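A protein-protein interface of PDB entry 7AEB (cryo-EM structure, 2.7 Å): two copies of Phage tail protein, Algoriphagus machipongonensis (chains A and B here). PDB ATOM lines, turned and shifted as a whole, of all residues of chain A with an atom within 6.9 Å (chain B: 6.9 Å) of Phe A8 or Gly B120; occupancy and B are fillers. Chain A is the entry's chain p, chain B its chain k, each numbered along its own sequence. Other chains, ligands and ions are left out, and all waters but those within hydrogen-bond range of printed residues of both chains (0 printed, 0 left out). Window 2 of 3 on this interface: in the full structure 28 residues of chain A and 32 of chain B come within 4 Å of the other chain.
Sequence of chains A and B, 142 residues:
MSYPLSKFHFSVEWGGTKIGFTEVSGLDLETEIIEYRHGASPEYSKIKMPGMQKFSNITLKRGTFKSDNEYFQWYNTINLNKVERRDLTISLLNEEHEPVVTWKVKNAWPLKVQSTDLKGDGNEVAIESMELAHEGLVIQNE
N of Gly B120 lies within hydrogen-bond range of O of Thr A22 (3.0 Å). The backbone carbonyl oxygen (O) of Glu B124 sits close to the backbone NH (N) of Lys A7. N of Leu B118 sits at hydrogen-bond distance from O of Val A24, at 3.0 Å.
Among the printed residues, pairs that only touch across the chains: Ser A6 with Glu B124 (3.8 Å), Lys A7 with Leu B118 (3.9 Å), Lys A7 with Lys B119 (3.6 Å), Lys A7 with Gly B122 (3.2 Å), Phe A8 with Lys B119 (3.4 Å), Phe A8 with Gly B120 (3.96 Å), Phe A8 with Gly B122 (3.8 Å), Phe A10 with Leu B118 (3.7 Å), Phe A10 with Lys B119 (3.97 Å), Thr A22 with Leu B118 (3.97 Å), Thr A22 with Lys B119 (3.6 Å) and Glu A23 with Leu B118 (3.4 Å).
Of chain B, only Lys B119, Gly B120 and Gly B122 come within 4 Å of Phe A8. Of the printed residues of chain B, Phe A10 touches Leu B118 and Lys B119. Of the printed residues of chain B, Glu A23 touches Leu B118. Printed residues of chain A within 4 Å of Lys B119: Lys A7 (3.6 Å), Phe A8 (3.4 Å), Phe A10 (3.97 Å) and Thr A22 (3.6 Å). Of chain A, only Phe A8 and Thr A22 come within 4 Å of Gly B120. The nearest residue of chain B that does not touch Phe A8 is Asn B123 (4.5 Å). The nearest residue of chain A that does not touch Gly B120 is Phe A10 (4.3 Å). The nearest printed residue of chain A that does not touch Gly B122 is Ser A6 (5.7 Å).
Hydrophobic or aromatic side chains of chain B that line the printed part of chain A: Leu B118. Printed residues of chain A that touch a printed residue of chain B: Ser A6, Lys A7, Phe A8, Phe A10, Thr A22, Glu A23 and Val A24. Hydrophobic or aromatic side chains of chain A that line the printed part of chain B: Phe A8 and Phe A10. Among the printed residues, no Asp or Glu carboxylate lies within 4 Å of a Lys or Arg side-chain nitrogen of the other chain.
No position is printed for both chains. Of the 15 pairs that touch across the chains among the printed residues, none has its exchanged pair printed and touching as well.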
ATOM      1  N   SER A   6       9.892  -8.644   0.935  1.00  0.00           N
ATOM      2  CA  SER A   6       9.386  -8.219  -0.370  1.00  0.00           C
ATOM      3  C   SER A   6      10.044  -9.044  -1.472  1.00  0.00           C
ATOM      4  O   SER A   6      10.951  -9.822  -1.201  1.00  0.00           O
ATOM      5  CB  SER A   6       9.616  -6.737  -0.587  1.00  0.00           C
ATOM      6  OG  SER A   6      10.974  -6.455  -0.720  1.00  0.00           O
ATOM      7  N   LYS A   7       9.596  -8.871  -2.726  1.00  0.00           N
ATOM      8  CA  LYS A   7      10.127  -9.708  -3.843  1.00  0.00           C
ATOM      9  C   LYS A   7      10.836  -8.924  -4.964  1.00  0.00           C
ATOM     10  O   LYS A   7      11.052  -9.543  -6.025  1.00  0.00           O
ATOM     11  CB  LYS A   7       8.991 -10.547  -4.439  1.00  0.00           C
ATOM     12  CG  LYS A   7       7.815  -9.751  -4.991  1.00  0.00           C
ATOM     13  CD  LYS A   7       6.703 -10.625  -5.532  1.00  0.00           C
ATOM     14  CE  LYS A   7       7.154 -11.534  -6.655  1.00  0.00           C
ATOM     15  NZ  LYS A   7       6.045 -12.376  -7.158  1.00  0.00           N
ATOM     16  N   PHE A   8      11.222  -7.655  -4.775  1.00  0.00           N
ATOM     17  CA  PHE A   8      11.854  -6.936  -5.889  1.00  0.00           C
ATOM     18  C   PHE A   8      13.357  -6.624  -5.819  1.00  0.00           C
ATOM     19  O   PHE A   8      13.909  -6.121  -6.790  1.00  0.00           O
ATOM     20  CB  PHE A   8      11.086  -5.639  -6.159  1.00  0.00           C
ATOM     21  CG  PHE A   8      11.016  -4.701  -5.006  1.00  0.00           C
ATOM     22  CD1 PHE A   8      12.037  -3.814  -4.739  1.00  0.00           C
ATOM     23  CD2 PHE A   8       9.912  -4.697  -4.186  1.00  0.00           C
ATOM     24  CE1 PHE A   8      11.958  -2.958  -3.683  1.00  0.00           C
ATOM     25  CE2 PHE A   8       9.832  -3.834  -3.128  1.00  0.00           C
ATOM     26  CZ  PHE A   8      10.857  -2.966  -2.877  1.00  0.00           C
ATOM     27  N   HIS A   9      14.032  -6.892  -4.710  1.00  0.00           N
ATOM     28  CA  HIS A   9      15.460  -6.581  -4.626  1.00  0.00           C
ATOM     29  C   HIS A   9      16.275  -7.884  -4.556  1.00  0.00           C
ATOM     30  O   HIS A   9      16.231  -8.600  -3.553  1.00  0.00           O
ATOM     31  CB  HIS A   9      15.697  -5.684  -3.414  1.00  0.00           C
ATOM     32  CG  HIS A   9      17.070  -5.154  -3.223  1.00  0.00           C
ATOM     33  ND1 HIS A   9      17.531  -4.820  -1.987  1.00  0.00           N
ATOM     34  CD2 HIS A   9      18.069  -4.849  -4.083  1.00  0.00           C
ATOM     35  CE1 HIS A   9      18.739  -4.364  -2.069  1.00  0.00           C
ATOM     36  NE2 HIS A   9      19.114  -4.360  -3.329  1.00  0.00           N
ATOM     37  N   PHE A  10      16.967  -8.209  -5.646  1.00  0.00           N
ATOM     38  CA  PHE A  10      17.684  -9.482  -5.774  1.00  0.00           C
ATOM     39  C   PHE A  10      18.837  -9.412  -6.768  1.00  0.00           C
ATOM     40  O   PHE A  10      18.920  -8.474  -7.559  1.00  0.00           O
ATOM     41  CB  PHE A  10      16.693 -10.585  -6.202  1.00  0.00           C
ATOM     42  CG  PHE A  10      16.023 -10.351  -7.543  1.00  0.00           C
ATOM     43  CD1 PHE A  10      16.557 -10.870  -8.714  1.00  0.00           C
ATOM     44  CD2 PHE A  10      14.861  -9.602  -7.628  1.00  0.00           C
ATOM     45  CE1 PHE A  10      15.952 -10.637  -9.927  1.00  0.00           C
ATOM     46  CE2 PHE A  10      14.260  -9.372  -8.835  1.00  0.00           C
ATOM     47  CZ  PHE A  10      14.804  -9.890  -9.995  1.00  0.00           C
ATOM     48  N   PHE A  21      18.724  -8.601 -13.427  1.00  0.00           N
ATOM     49  CA  PHE A  21      17.687  -9.268 -14.205  1.00  0.00           C
ATOM     50  C   PHE A  21      16.331  -8.664 -13.961  1.00  0.00           C
ATOM     51  O   PHE A  21      16.080  -8.083 -12.909  1.00  0.00           O
ATOM     52  CB  PHE A  21      17.673 -10.780 -13.931  1.00  0.00           C
ATOM     53  CG  PHE A  21      18.867 -11.503 -14.489  1.00  0.00           C
ATOM     54  CD1 PHE A  21      20.095 -11.487 -13.881  1.00  0.00           C
ATOM     55  CD2 PHE A  21      18.736 -12.226 -15.649  1.00  0.00           C
ATOM     56  CE1 PHE A  21      21.159 -12.146 -14.430  1.00  0.00           C
ATOM     57  CE2 PHE A  21      19.805 -12.895 -16.187  1.00  0.00           C
ATOM     58  CZ  PHE A  21      21.010 -12.848 -15.579  1.00  0.00           C
ATOM     59  N   THR A  22      15.460  -8.808 -14.938  1.00  0.00           N
ATOM     60  CA  THR A  22      14.088  -8.356 -14.854  1.00  0.00           C
ATOM     61  C   THR A  22      13.208  -9.393 -14.165  1.00  0.00           C
ATOM     62  O   THR A  22      12.346  -9.053 -13.357  1.00  0.00           O
ATOM     63  CB  THR A  22      13.537  -7.984 -16.258  1.00  0.00           C
ATOM     64  OG1 THR A  22      14.280  -6.871 -16.806  1.00  0.00           O
ATOM     65  CG2 THR A  22      12.106  -7.598 -16.175  1.00  0.00           C
ATOM     66  N   GLU A  23      13.410 -10.660 -14.503  1.00  0.00           N
ATOM     67  CA  GLU A  23      12.570 -11.723 -13.968  1.00  0.00           C
ATOM     68  C   GLU A  23      13.298 -13.051 -13.781  1.00  0.00           C
ATOM     69  O   GLU A  23      14.128 -13.444 -14.604  1.00  0.00           O
ATOM     70  CB  GLU A  23      11.364 -11.935 -14.880  1.00  0.00           C
ATOM     71  CG  GLU A  23      10.345 -12.953 -14.395  1.00  0.00           C
ATOM     72  CD  GLU A  23       9.170 -13.103 -15.328  1.00  0.00           C
ATOM     73  OE1 GLU A  23       9.014 -12.298 -16.223  1.00  0.00           O
ATOM     74  OE2 GLU A  23       8.427 -14.032 -15.159  1.00  0.00           O
ATOM     75  N   VAL A  24      13.001 -13.727 -12.664  1.00  0.00           N
ATOM     76  CA  VAL A  24      13.520 -15.061 -12.351  1.00  0.00           C
ATOM     77  C   VAL A  24      12.375 -15.998 -11.931  1.00  0.00           C
ATOM     78  O   VAL A  24      11.623 -15.667 -11.016  1.00  0.00           O
ATOM     79  CB  VAL A  24      14.554 -14.993 -11.192  1.00  0.00           C
ATOM     80  CG1 VAL A  24      15.097 -16.402 -10.857  1.00  0.00           C
ATOM     81  CG2 VAL A  24      15.688 -14.045 -11.552  1.00  0.00           C
ATOM     82  N   LEU A  92      18.259 -13.208  -2.612  1.00  0.00           N
ATOM     83  CA  LEU A  92      17.315 -12.178  -2.142  1.00  0.00           C
ATOM     84  C   LEU A  92      18.066 -11.285  -1.169  1.00  0.00           C
ATOM     85  O   LEU A  92      18.684 -11.791  -0.222  1.00  0.00           O
ATOM     86  CB  LEU A  92      16.108 -12.847  -1.468  1.00  0.00           C
ATOM     87  CG  LEU A  92      14.914 -11.966  -1.038  1.00  0.00           C
ATOM     88  CD1 LEU A  92      13.664 -12.824  -1.040  1.00  0.00           C
ATOM     89  CD2 LEU A  92      15.143 -11.408   0.382  1.00  0.00           C
ATOM     90  N   LEU B 118      10.586 -13.800  -8.883  1.00  0.00           N
ATOM     91  CA  LEU B 118      11.142 -12.490  -8.609  1.00  0.00           C
ATOM     92  C   LEU B 118      10.884 -11.546  -9.766  1.00  0.00           C
ATOM     93  O   LEU B 118      11.073 -11.922 -10.920  1.00  0.00           O
ATOM     94  CB  LEU B 118      12.642 -12.660  -8.365  1.00  0.00           C
ATOM     95  CG  LEU B 118      13.036 -13.659  -7.223  1.00  0.00           C
ATOM     96  CD1 LEU B 118      14.522 -13.846  -7.216  1.00  0.00           C
ATOM     97  CD2 LEU B 118      12.576 -13.140  -5.879  1.00  0.00           C
ATOM     98  N   LYS B 119      10.460 -10.319  -9.468  1.00  0.00           N
ATOM     99  CA  LYS B 119      10.199  -9.329 -10.507  1.00  0.00           C
ATOM    100  C   LYS B 119      10.724  -7.948 -10.145  1.00  0.00           C
ATOM    101  O   LYS B 119      10.557  -7.492  -9.017  1.00  0.00           O
ATOM    102  CB  LYS B 119       8.702  -9.235 -10.774  1.00  0.00           C
ATOM    103  CG  LYS B 119       8.084 -10.479 -11.328  1.00  0.00           C
ATOM    104  CD  LYS B 119       6.620 -10.282 -11.611  1.00  0.00           C
ATOM    105  CE  LYS B 119       6.007 -11.546 -12.172  1.00  0.00           C
ATOM    106  NZ  LYS B 119       4.552 -11.400 -12.424  1.00  0.00           N
ATOM    107  N   GLY B 120      11.303  -7.254 -11.128  1.00  0.00           N
ATOM    108  CA  GLY B 120      11.841  -5.897 -10.951  1.00  0.00           C
ATOM    109  C   GLY B 120      10.808  -4.875 -10.487  1.00  0.00           C
ATOM    110  O   GLY B 120      11.128  -3.954  -9.741  1.00  0.00           O
ATOM    111  N   ASP B 121       9.572  -5.040 -10.929  1.00  0.00           N
ATOM    112  CA  ASP B 121       8.454  -4.196 -10.574  1.00  0.00           C
ATOM    113  C   ASP B 121       7.422  -4.948  -9.723  1.00  0.00           C
ATOM    114  O   ASP B 121       6.255  -4.557  -9.615  1.00  0.00           O
ATOM    115  CB  ASP B 121       7.881  -3.611 -11.851  1.00  0.00           C
ATOM    116  CG  ASP B 121       7.505  -4.683 -12.832  1.00  0.00           C
ATOM    117  OD1 ASP B 121       7.923  -5.819 -12.624  1.00  0.00           O
ATOM    118  OD2 ASP B 121       6.841  -4.393 -13.793  1.00  0.00           O
ATOM    119  N   GLY B 122       7.868  -6.010  -9.066  1.00  0.00           N
ATOM    120  CA  GLY B 122       7.021  -6.856  -8.245  1.00  0.00           C
ATOM    121  C   GLY B 122       6.722  -6.286  -6.880  1.00  0.00           C
ATOM    122  O   GLY B 122       7.239  -6.763  -5.874  1.00  0.00           O
ATOM    123  N   ASN B 123       5.870  -5.284  -6.836  1.00  0.00           N
ATOM    124  CA  ASN B 123       5.525  -4.628  -5.576  1.00  0.00           C
ATOM    125  C   ASN B 123       4.542  -5.453  -4.736  1.00  0.00           C
ATOM    126  O   ASN B 123       3.389  -5.061  -4.571  1.00  0.00           O
ATOM    127  CB  ASN B 123       4.926  -3.261  -5.852  1.00  0.00           C
ATOM    128  CG  ASN B 123       4.799  -2.412  -4.630  1.00  0.00           C
ATOM    129  OD1 ASN B 123       5.617  -2.505  -3.715  1.00  0.00           O
ATOM    130  ND2 ASN B 123       3.792  -1.592  -4.590  1.00  0.00           N
ATOM    131  N   GLU B 124       5.008  -6.592  -4.214  1.00  0.00           N
ATOM    132  CA  GLU B 124       4.160  -7.513  -3.443  1.00  0.00           C
ATOM    133  C   GLU B 124       4.978  -8.360  -2.444  1.00  0.00           C
ATOM    134  O   GLU B 124       6.204  -8.284  -2.414  1.00  0.00           O
ATOM    135  CB  GLU B 124       3.387  -8.377  -4.482  1.00  0.00           C
ATOM    136  CG  GLU B 124       2.383  -9.472  -3.990  1.00  0.00           C
ATOM    137  CD  GLU B 124       1.255  -8.975  -3.113  1.00  0.00           C
ATOM    138  OE1 GLU B 124       0.160  -8.794  -3.578  1.00  0.00           O
ATOM    139  OE2 GLU B 124       1.531  -8.773  -1.963  1.00  0.00           O
